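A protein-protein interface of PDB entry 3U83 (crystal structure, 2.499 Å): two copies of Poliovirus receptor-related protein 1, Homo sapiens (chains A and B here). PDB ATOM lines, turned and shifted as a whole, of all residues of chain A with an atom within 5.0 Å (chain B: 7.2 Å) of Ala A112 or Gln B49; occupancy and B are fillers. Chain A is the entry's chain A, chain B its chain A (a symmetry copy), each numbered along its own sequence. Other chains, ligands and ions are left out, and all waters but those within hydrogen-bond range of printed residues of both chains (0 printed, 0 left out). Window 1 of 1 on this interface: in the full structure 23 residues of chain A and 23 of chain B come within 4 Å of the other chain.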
ATOM      1  N   LYS A  46      24.092  -9.195 -37.571  1.00  0.00           N
ATOM      2  CA  LYS A  46      24.600 -10.545 -37.362  1.00  0.00           C
ATOM      3  C   LYS A  46      24.089 -11.125 -36.050  1.00  0.00           C
ATOM      4  O   LYS A  46      24.118 -10.462 -35.012  1.00  0.00           O
ATOM      5  CB  LYS A  46      26.126 -10.565 -37.383  1.00  0.00           C
ATOM      6  CG  LYS A  46      26.723 -11.915 -37.043  1.00  0.00           C
ATOM      7  CD  LYS A  46      28.222 -11.928 -37.285  1.00  0.00           C
ATOM      8  CE  LYS A  46      28.802 -13.323 -37.100  1.00  0.00           C
ATOM      9  NZ  LYS A  46      30.251 -13.370 -37.450  1.00  0.00           N
ATOM     10  N   ILE A  47      23.610 -12.362 -36.105  1.00  0.00           N
ATOM     11  CA  ILE A  47      23.070 -13.021 -34.925  1.00  0.00           C
ATOM     12  C   ILE A  47      24.177 -13.680 -34.118  1.00  0.00           C
ATOM     13  O   ILE A  47      24.935 -14.507 -34.617  1.00  0.00           O
ATOM     14  CB  ILE A  47      21.979 -14.056 -35.277  1.00  0.00           C
ATOM     15  CG1 ILE A  47      20.652 -13.353 -35.560  1.00  0.00           C
ATOM     16  CG2 ILE A  47      21.786 -15.039 -34.135  1.00  0.00           C
ATOM     17  CD1 ILE A  47      20.662 -12.505 -36.804  1.00  0.00           C
ATOM     18  N   THR A  48      24.246 -13.305 -32.852  1.00  0.00           N
ATOM     19  CA  THR A  48      25.324 -13.717 -31.981  1.00  0.00           C
ATOM     20  C   THR A  48      24.976 -14.986 -31.223  1.00  0.00           C
ATOM     21  O   THR A  48      25.802 -15.887 -31.079  1.00  0.00           O
ATOM     22  CB  THR A  48      25.602 -12.615 -30.957  1.00  0.00           C
ATOM     23  OG1 THR A  48      26.032 -11.437 -31.641  1.00  0.00           O
ATOM     24  CG2 THR A  48      26.673 -13.040 -30.009  1.00  0.00           C
ATOM     25  N   GLN A  49      23.739 -15.048 -30.747  1.00  0.00           N
ATOM     26  CA  GLN A  49      23.340 -16.095 -29.826  1.00  0.00           C
ATOM     27  C   GLN A  49      21.829 -16.043 -29.625  1.00  0.00           C
ATOM     28  O   GLN A  49      21.228 -14.969 -29.641  1.00  0.00           O
ATOM     29  CB  GLN A  49      24.074 -15.890 -28.499  1.00  0.00           C
ATOM     30  CG  GLN A  49      23.836 -16.944 -27.448  1.00  0.00           C
ATOM     31  CD  GLN A  49      24.908 -16.909 -26.366  1.00  0.00           C
ATOM     32  OE1 GLN A  49      26.103 -17.000 -26.655  1.00  0.00           O
ATOM     33  NE2 GLN A  49      24.486 -16.786 -25.117  1.00  0.00           N
ATOM     34  N   GLU A 110      15.432 -14.793 -26.671  1.00  0.00           N
ATOM     35  CA  GLU A 110      16.183 -13.601 -27.001  1.00  0.00           C
ATOM     36  C   GLU A 110      17.231 -13.849 -28.081  1.00  0.00           C
ATOM     37  O   GLU A 110      18.042 -14.769 -27.978  1.00  0.00           O
ATOM     38  CB  GLU A 110      16.826 -13.037 -25.742  1.00  0.00           C
ATOM     39  CG  GLU A 110      17.659 -11.810 -25.981  1.00  0.00           C
ATOM     40  CD  GLU A 110      18.597 -11.544 -24.829  1.00  0.00           C
ATOM     41  OE1 GLU A 110      19.822 -11.774 -24.980  1.00  0.00           O
ATOM     42  OE2 GLU A 110      18.094 -11.128 -23.763  1.00  0.00           O
ATOM     43  N   PHE A 111      17.179 -13.030 -29.126  1.00  0.00           N
ATOM     44  CA  PHE A 111      18.211 -12.992 -30.151  1.00  0.00           C
ATOM     45  C   PHE A 111      19.161 -11.848 -29.838  1.00  0.00           C
ATOM     46  O   PHE A 111      18.770 -10.681 -29.840  1.00  0.00           O
ATOM     47  CB  PHE A 111      17.596 -12.766 -31.537  1.00  0.00           C
ATOM     48  CG  PHE A 111      16.993 -14.000 -32.153  1.00  0.00           C
ATOM     49  CD1 PHE A 111      17.735 -14.792 -33.015  1.00  0.00           C
ATOM     50  CD2 PHE A 111      15.684 -14.361 -31.881  1.00  0.00           C
ATOM     51  CE1 PHE A 111      17.189 -15.921 -33.589  1.00  0.00           C
ATOM     52  CE2 PHE A 111      15.129 -15.496 -32.452  1.00  0.00           C
ATOM     53  CZ  PHE A 111      15.884 -16.277 -33.307  1.00  0.00           C
ATOM     54  N   ALA A 112      20.408 -12.187 -29.543  1.00  0.00           N
ATOM     55  CA  ALA A 112      21.445 -11.183 -29.410  1.00  0.00           C
ATOM     56  C   ALA A 112      22.065 -10.986 -30.789  1.00  0.00           C
ATOM     57  O   ALA A 112      22.446 -11.951 -31.450  1.00  0.00           O
ATOM     58  CB  ALA A 112      22.484 -11.639 -28.412  1.00  0.00           C
ATOM     59  N   THR A 113      22.142  -9.738 -31.232  1.00  0.00           N
ATOM     60  CA  THR A 113      22.663  -9.431 -32.554  1.00  0.00           C
ATOM     61  C   THR A 113      23.644  -8.276 -32.456  1.00  0.00           C
ATOM     62  O   THR A 113      23.641  -7.529 -31.478  1.00  0.00           O
ATOM     63  CB  THR A 113      21.530  -9.027 -33.528  1.00  0.00           C
ATOM     64  OG1 THR A 113      21.061  -7.711 -33.203  1.00  0.00           O
ATOM     65  CG2 THR A 113      20.365 -10.003 -33.436  1.00  0.00           C
ATOM     66  N   PHE A 114      24.478  -8.134 -33.479  1.00  0.00           N
ATOM     67  CA  PHE A 114      25.428  -7.034 -33.565  1.00  0.00           C
ATOM     68  C   PHE A 114      25.352  -6.423 -34.962  1.00  0.00           C
ATOM     69  O   PHE A 114      25.306  -7.146 -35.956  1.00  0.00           O
ATOM     70  CB  PHE A 114      26.850  -7.522 -33.263  1.00  0.00           C
ATOM     71  CG  PHE A 114      27.817  -6.414 -32.982  1.00  0.00           C
ATOM     72  CD1 PHE A 114      27.962  -5.914 -31.695  1.00  0.00           C
ATOM     73  CD2 PHE A 114      28.570  -5.854 -34.005  1.00  0.00           C
ATOM     74  CE1 PHE A 114      28.849  -4.878 -31.435  1.00  0.00           C
ATOM     75  CE2 PHE A 114      29.458  -4.815 -33.752  1.00  0.00           C
ATOM     76  CZ  PHE A 114      29.598  -4.329 -32.468  1.00  0.00           C
ATOM     77  N   GLY A 117      21.850  -5.168 -31.318  1.00  0.00           N
ATOM     78  CA  GLY A 117      21.481  -5.521 -29.959  1.00  0.00           C
ATOM     79  C   GLY A 117      20.430  -6.611 -29.813  1.00  0.00           C
ATOM     80  O   GLY A 117      20.268  -7.469 -30.684  1.00  0.00           O
ATOM     81  N   ASN A 118      19.707  -6.573 -28.700  1.00  0.00           N
ATOM     82  CA  ASN A 118      18.793  -7.650 -28.351  1.00  0.00           C
ATOM     83  C   ASN A 118      17.383  -7.532 -28.911  1.00  0.00           C
ATOM     84  O   ASN A 118      16.829  -6.441 -29.035  1.00  0.00           O
ATOM     85  CB  ASN A 118      18.717  -7.806 -26.833  1.00  0.00           C
ATOM     86  CG  ASN A 118      19.900  -8.566 -26.268  1.00  0.00           C
ATOM     87  OD1 ASN A 118      20.869  -8.841 -26.979  1.00  0.00           O
ATOM     88  ND2 ASN A 118      19.833  -8.904 -24.983  1.00  0.00           N
ATOM     89  N   LYS B  46      32.253 -18.567 -21.357  1.00  0.00           N
ATOM     90  CA  LYS B  46      32.775 -17.580 -22.294  1.00  0.00           C
ATOM     91  C   LYS B  46      31.767 -16.465 -22.532  1.00  0.00           C
ATOM     92  O   LYS B  46      30.581 -16.720 -22.753  1.00  0.00           O
ATOM     93  CB  LYS B  46      33.155 -18.232 -23.622  1.00  0.00           C
ATOM     94  CG  LYS B  46      33.582 -17.244 -24.687  1.00  0.00           C
ATOM     95  CD  LYS B  46      34.147 -17.957 -25.903  1.00  0.00           C
ATOM     96  CE  LYS B  46      34.724 -16.971 -26.907  1.00  0.00           C
ATOM     97  NZ  LYS B  46      35.384 -17.667 -28.048  1.00  0.00           N
ATOM     98  N   ILE B  47      32.241 -15.227 -22.474  1.00  0.00           N
ATOM     99  CA  ILE B  47      31.374 -14.071 -22.659  1.00  0.00           C
ATOM    100  C   ILE B  47      31.213 -13.745 -24.136  1.00  0.00           C
ATOM    101  O   ILE B  47      32.182 -13.527 -24.858  1.00  0.00           O
ATOM    102  CB  ILE B  47      31.878 -12.829 -21.892  1.00  0.00           C
ATOM    103  CG1 ILE B  47      31.512 -12.935 -20.412  1.00  0.00           C
ATOM    104  CG2 ILE B  47      31.265 -11.562 -22.464  1.00  0.00           C
ATOM    105  CD1 ILE B  47      32.229 -14.040 -19.682  1.00  0.00           C
ATOM    106  N   THR B  48      29.964 -13.705 -24.567  1.00  0.00           N
ATOM    107  CA  THR B  48      29.633 -13.556 -25.967  1.00  0.00           C
ATOM    108  C   THR B  48      29.444 -12.098 -26.344  1.00  0.00           C
ATOM    109  O   THR B  48      29.901 -11.649 -27.396  1.00  0.00           O
ATOM    110  CB  THR B  48      28.328 -14.295 -26.264  1.00  0.00           C
ATOM    111  OG1 THR B  48      28.512 -15.691 -26.014  1.00  0.00           O
ATOM    112  CG2 THR B  48      27.934 -14.109 -27.692  1.00  0.00           C
ATOM    113  N   GLN B  49      28.770 -11.362 -25.470  1.00  0.00           N
ATOM    114  CA  GLN B  49      28.331 -10.020 -25.797  1.00  0.00           C
ATOM    115  C   GLN B  49      27.783  -9.346 -24.543  1.00  0.00           C
ATOM    116  O   GLN B  49      27.193  -9.999 -23.684  1.00  0.00           O
ATOM    117  CB  GLN B  49      27.257 -10.104 -26.884  1.00  0.00           C
ATOM    118  CG  GLN B  49      26.744  -8.785 -27.404  1.00  0.00           C
ATOM    119  CD  GLN B  49      26.034  -8.949 -28.742  1.00  0.00           C
ATOM    120  OE1 GLN B  49      26.601  -9.479 -29.699  1.00  0.00           O
ATOM    121  NE2 GLN B  49      24.795  -8.486 -28.816  1.00  0.00           N
ATOM    122  N   VAL B  50      27.995  -8.041 -24.445  1.00  0.00           N
ATOM    123  CA  VAL B  50      27.511  -7.252 -23.329  1.00  0.00           C
ATOM    124  C   VAL B  50      26.558  -6.214 -23.894  1.00  0.00           C
ATOM    125  O   VAL B  50      26.911  -5.482 -24.817  1.00  0.00           O
ATOM    126  CB  VAL B  50      28.677  -6.529 -22.617  1.00  0.00           C
ATOM    127  CG1 VAL B  50      28.164  -5.661 -21.483  1.00  0.00           C
ATOM    128  CG2 VAL B  50      29.690  -7.540 -22.108  1.00  0.00           C
ATOM    129  N   THR B  51      25.355  -6.143 -23.335  1.00  0.00           N
ATOM    130  CA  THR B  51      24.302  -5.309 -23.905  1.00  0.00           C
ATOM    131  C   THR B  51      23.615  -4.411 -22.875  1.00  0.00           C
ATOM    132  O   THR B  51      23.114  -4.884 -21.850  1.00  0.00           O
ATOM    133  CB  THR B  51      23.237  -6.180 -24.600  1.00  0.00           C
ATOM    134  OG1 THR B  51      23.876  -7.030 -25.558  1.00  0.00           O
ATOM    135  CG2 THR B  51      22.215  -5.309 -25.310  1.00  0.00           C
ATOM    136  N   ASN B  62      17.563  -0.784 -27.265  1.00  0.00           N
ATOM    137  CA  ASN B  62      18.996  -1.001 -27.138  1.00  0.00           C
ATOM    138  C   ASN B  62      19.780   0.303 -27.090  1.00  0.00           C
ATOM    139  O   ASN B  62      19.537   1.215 -27.883  1.00  0.00           O
ATOM    140  CB  ASN B  62      19.505  -1.889 -28.270  1.00  0.00           C
ATOM    141  CG  ASN B  62      18.921  -3.281 -28.217  1.00  0.00           C
ATOM    142  OD1 ASN B  62      19.351  -4.114 -27.419  1.00  0.00           O
ATOM    143  ND2 ASN B  62      17.930  -3.541 -29.066  1.00  0.00           N
ATOM    144  N   ILE B  65      26.183  -1.817 -27.282  1.00  0.00           N
ATOM    145  CA  ILE B  65      26.613  -3.205 -27.295  1.00  0.00           C
ATOM    146  C   ILE B  65      28.130  -3.305 -27.369  1.00  0.00           C
ATOM    147  O   ILE B  65      28.787  -2.563 -28.106  1.00  0.00           O
ATOM    148  CB  ILE B  65      26.019  -3.983 -28.501  1.00  0.00           C
ATOM    149  CG1 ILE B  65      24.492  -3.943 -28.491  1.00  0.00           C
ATOM    150  CG2 ILE B  65      26.484  -5.429 -28.486  1.00  0.00           C
ATOM    151  CD1 ILE B  65      23.916  -2.684 -29.061  1.00  0.00           C
ATOM    152  N   TYR B  66      28.689  -4.230 -26.603  1.00  0.00           N
ATOM    153  CA  TYR B  66      30.093  -4.571 -26.753  1.00  0.00           C
ATOM    154  C   TYR B  66      30.251  -6.056 -27.019  1.00  0.00           C
ATOM    155  O   TYR B  66      29.852  -6.896 -26.208  1.00  0.00           O
ATOM    156  CB  TYR B  66      30.903  -4.178 -25.522  1.00  0.00           C
ATOM    157  CG  TYR B  66      32.278  -4.802 -25.502  1.00  0.00           C
ATOM    158  CD1 TYR B  66      33.316  -4.273 -26.261  1.00  0.00           C
ATOM    159  CD2 TYR B  66      32.535  -5.928 -24.733  1.00  0.00           C
ATOM    160  CE1 TYR B  66      34.574  -4.846 -26.246  1.00  0.00           C
ATOM    161  CE2 TYR B  66      33.789  -6.505 -24.711  1.00  0.00           C
ATOM    162  CZ  TYR B  66      34.803  -5.962 -25.466  1.00  0.00           C
ATOM    163  OH  TYR B  66      36.048  -6.544 -25.440  1.00  0.00           O
ATOM    164  N   ASN B  67      30.835  -6.368 -28.168  1.00  0.00           N
ATOM    165  CA  ASN B  67      31.106  -7.740 -28.563  1.00  0.00           C
ATOM    166  C   ASN B  67      32.609  -7.908 -28.779  1.00  0.00           C
ATOM    167  O   ASN B  67      33.195  -7.233 -29.619  1.00  0.00           O
ATOM    168  CB  ASN B  67      30.328  -8.074 -29.836  1.00  0.00           C
ATOM    169  CG  ASN B  67      30.524  -9.507 -30.294  1.00  0.00           C
ATOM    170  OD1 ASN B  67      31.646  -9.949 -30.553  1.00  0.00           O
ATOM    171  ND2 ASN B  67      29.422 -10.238 -30.413  1.00  0.00           N
ATOM    172  N   PRO B  68      33.238  -8.802 -28.005  1.00  0.00           N
ATOM    173  CA  PRO B  68      34.691  -9.004 -28.037  1.00  0.00           C
ATOM    174  C   PRO B  68      35.223  -9.273 -29.442  1.00  0.00           C
ATOM    175  O   PRO B  68      36.356  -8.895 -29.748  1.00  0.00           O
ATOM    176  CB  PRO B  68      34.892 -10.243 -27.157  1.00  0.00           C
ATOM    177  CG  PRO B  68      33.740 -10.235 -26.239  1.00  0.00           C
ATOM    178  CD  PRO B  68      32.579  -9.686 -27.029  1.00  0.00           C
ATOM    179  N   MET B  70      33.700  -8.282 -32.416  1.00  0.00           N
ATOM    180  CA  MET B  70      33.347  -7.278 -33.414  1.00  0.00           C
ATOM    181  C   MET B  70      33.462  -5.833 -32.929  1.00  0.00           C
ATOM    182  O   MET B  70      33.303  -4.902 -33.710  1.00  0.00           O
ATOM    183  CB  MET B  70      31.951  -7.560 -33.966  1.00  0.00           C
ATOM    184  CG  MET B  70      31.874  -8.871 -34.740  1.00  0.00           C
ATOM    185  SD  MET B  70      30.200  -9.531 -34.868  1.00  0.00           S
ATOM    186  CE  MET B  70      29.434  -8.306 -35.920  1.00  0.00           C
ATOM    187  N   GLU B 110      23.190  -6.721 -19.725  1.00  0.00           N
ATOM    188  CA  GLU B 110      23.134  -8.158 -19.886  1.00  0.00           C
ATOM    189  C   GLU B 110      24.423  -8.734 -20.460  1.00  0.00           C
ATOM    190  O   GLU B 110      24.921  -8.275 -21.487  1.00  0.00           O
ATOM    191  CB  GLU B 110      21.941  -8.528 -20.757  1.00  0.00           C
ATOM    192  CG  GLU B 110      21.809 -10.003 -21.013  1.00  0.00           C
ATOM    193  CD  GLU B 110      20.908 -10.281 -22.191  1.00  0.00           C
ATOM    194  OE1 GLU B 110      21.422 -10.664 -23.270  1.00  0.00           O
ATOM    195  OE2 GLU B 110      19.683 -10.088 -22.035  1.00  0.00           O
ATOM    196  N   PHE B 111      24.967  -9.726 -19.761  1.00  0.00           N
ATOM    197  CA  PHE B 111      26.080 -10.521 -20.254  1.00  0.00           C
ATOM    198  C   PHE B 111      25.531 -11.806 -20.850  1.00  0.00           C
ATOM    199  O   PHE B 111      24.936 -12.625 -20.151  1.00  0.00           O
ATOM    200  CB  PHE B 111      27.047 -10.871 -19.116  1.00  0.00           C
ATOM    201  CG  PHE B 111      27.980  -9.753 -18.733  1.00  0.00           C
ATOM    202  CD1 PHE B 111      29.245  -9.669 -19.292  1.00  0.00           C
ATOM    203  CD2 PHE B 111      27.597  -8.796 -17.809  1.00  0.00           C
ATOM    204  CE1 PHE B 111      30.110  -8.652 -18.942  1.00  0.00           C
ATOM    205  CE2 PHE B 111      28.459  -7.768 -17.455  1.00  0.00           C
ATOM    206  CZ  PHE B 111      29.716  -7.697 -18.024  1.00  0.00           C
ATOM    207  N   ALA B 112      25.710 -11.970 -22.154  1.00  0.00           N
ATOM    208  CA  ALA B 112      25.398 -13.229 -22.800  1.00  0.00           C
ATOM    209  C   ALA B 112      26.656 -14.089 -22.749  1.00  0.00           C
ATOM    210  O   ALA B 112      27.738 -13.639 -23.122  1.00  0.00           O
ATOM    211  CB  ALA B 112      24.968 -12.988 -24.228  1.00  0.00           C
ATOM    212  N   THR B 113      26.518 -15.315 -22.263  1.00  0.00           N
ATOM    213  CA  THR B 113      27.657 -16.207 -22.114  1.00  0.00           C
ATOM    214  C   THR B 113      27.297 -17.581 -22.651  1.00  0.00           C
ATOM    215  O   THR B 113      26.120 -17.912 -22.796  1.00  0.00           O
ATOM    216  CB  THR B 113      28.068 -16.357 -20.630  1.00  0.00           C
ATOM    217  OG1 THR B 113      27.105 -17.168 -19.941  1.00  0.00           O
ATOM    218  CG2 THR B 113      28.142 -14.996 -19.949  1.00  0.00           C
ATOM    219  N   ASN B 118      22.377 -16.162 -20.145  1.00  0.00           N
ATOM    220  CA  ASN B 118      22.329 -14.746 -19.813  1.00  0.00           C
ATOM    221  C   ASN B 118      22.440 -14.405 -18.334  1.00  0.00           C
ATOM    222  O   ASN B 118      21.946 -15.127 -17.468  1.00  0.00           O
ATOM    223  CB  ASN B 118      21.058 -14.114 -20.378  1.00  0.00           C
ATOM    224  CG  ASN B 118      21.169 -13.811 -21.858  1.00  0.00           C
ATOM    225  OD1 ASN B 118      22.132 -14.217 -22.513  1.00  0.00           O
ATOM    226  ND2 ASN B 118      20.182 -13.101 -22.398  1.00  0.00           N
ATOM    227  N   ARG B 119      23.096 -13.285 -18.065  1.00  0.00           N
ATOM    228  CA  ARG B 119      23.226 -12.759 -16.722  1.00  0.00           C
ATOM    229  C   ARG B 119      22.894 -11.279 -16.809  1.00  0.00           C
ATOM    230  O   ARG B 119      23.580 -10.537 -17.508  1.00  0.00           O
ATOM    231  CB  ARG B 119      24.664 -12.932 -16.241  1.00  0.00           C
ATOM    232  CG  ARG B 119      24.790 -13.141 -14.750  1.00  0.00           C
ATOM    233  CD  ARG B 119      25.809 -12.198 -14.124  1.00  0.00           C
ATOM    234  NE  ARG B 119      27.067 -12.844 -13.743  1.00  0.00           N
ATOM    235  CZ  ARG B 119      27.174 -14.033 -13.145  1.00  0.00           C
ATOM    236  NH1 ARG B 119      26.096 -14.748 -12.855  1.00  0.00           N
ATOM    237  NH2 ARG B 119      28.375 -14.511 -12.839  1.00  0.00           N
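OE1 of Gln A49 is in hydrogen-bond range of OG1 of Thr B48, at 2.8 Å.
ND2 of Asn A118 lies within hydrogen-bond range of OE1 of Glu B110 (2.9 Å).
The side-chain amide oxygen of Asn B62 lies within hydrogen-bond range of the backbone NH of Asn A118, at 2.8 Å.
The side-chain carboxylate (OE1) of Glu A110 lies within hydrogen-bond range of the side-chain amide nitrogen (ND2) of Asn B118 (2.9 Å).
OG1 of Thr A48 is in hydrogen-bond range of OE1 of Gln B49, 2.8 Å away.
The backbone carbonyl oxygen of Thr A113 sits at hydrogen-bond distance from the side-chain amide nitrogen of Gln B49 (3.1 Å).
The side-chain carboxylate of Glu B110 sits close to the side-chain carboxylate of Glu A110 (2.6 Å).
The side-chain amide nitrogen of Gln A49 sits at hydrogen-bond distance from the backbone carbonyl oxygen of Thr B113.
The side-chain amide nitrogen (ND2) of Asn B118 lies within hydrogen-bond range of the side-chain carboxylate (OE1) of Glu B110.
O of Gln B49 is in hydrogen-bond range of N of Ala B112, 2.9 Å away.
The side-chain amide oxygen of Asn B67 sits at hydrogen-bond distance from the backbone NH of Met B70, 3.2 Å away.
O of Lys A46 lies within hydrogen-bond range of N of Phe A114 (2.8 Å).
The side-chain amide nitrogen of Asn B67 lies within hydrogen-bond range of the backbone carbonyl oxygen of Thr B48, at 3.4 Å.
The side-chain amide oxygen of Gln B49 is in hydrogen-bond range of the side-chain amide nitrogen of Asn B67.
Among the printed residues, pairs that only touch across the chains: Lys A46 with Met B70 (3.9 Å), Thr A48 with Thr B48 (2.8 Å), Thr A48 with Asn B67 (3.8 Å), Gln A49 with Ala B112 (3.9 Å), Ala A112 with Gln B49 (3.9 Å), Phe A114 with Ile B65 (3.6 Å), Phe A114 with Asn B67 (3.7 Å), Phe A114 with Met B70 (3.2 Å), Gly A117 with Asn B62 (3.6 Å), Gly A117 with Ile B65 (3.7 Å) and Asn A118 with Thr B51 (3.8 Å).
Ala A112 touches just one residue of chain B: Gln B49 (3.9 Å).
Gln B49 touches just these residues of chain A: Thr A48, Ala A112 and Thr A113.
Of the printed residues of chain A, Ala B112 touches Gln A49 (3.9 Å).
Of the printed residues of chain B, Asn A118 touches Thr B51, Asn B62 and Glu B110.
Of the printed residues of chain A, Thr B113 touches Gln A49.
Of the printed residues of chain B, Phe A114 touches Ile B65 (3.6 Å), Asn B67 (3.7 Å) and Met B70 (3.2 Å).
Lys B46 touches none of the printed residues of chain A.
Phe A111 touches none of the printed residues of chain B.
The nearest residue of chain B that does not touch Ala A112 is Ala B112 (5.0 Å).
The nearest printed residue of chain B that does not touch Gln A49 is Asn B118 (4.3 Å).
Of the 18 printed residues of chain B, 11 touch a printed residue of chain A.
Hydrophobic or aromatic side chains of chain B that line the printed part of chain A: Ile B65, Met B70 and Ala B112.
Printed residues of chain A that touch a printed residue of chain B: Lys A46, Thr A48, Gln A49, Glu A110, Ala A112, Thr A113, Phe A114, Gly A117 and Asn A118.
Hydrophobic or aromatic side chains of chain A within 4 Å of the printed part of chain B: Ala A112 and Phe A114.
Among the printed residues, 19 pairs touch across the chains.
Among the printed residues, no Asp or Glu carboxylate lies within 4 Å of a Lys or Arg side-chain nitrogen of the other chain.
Thr B48 touches its own counterpart, Thr A48.
Gln A49 touches Ala B112, and with the chains exchanged Ala A112 touches Gln B49.
Glu B110 touches its own counterpart, Glu A110.
Glu A110 touches Asn B118, and with the chains exchanged Asn A118 touches Glu B110.
Of the 19 pairs that touch across the chains among the printed residues, 10 have their exchanged pair printed and touching as well.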
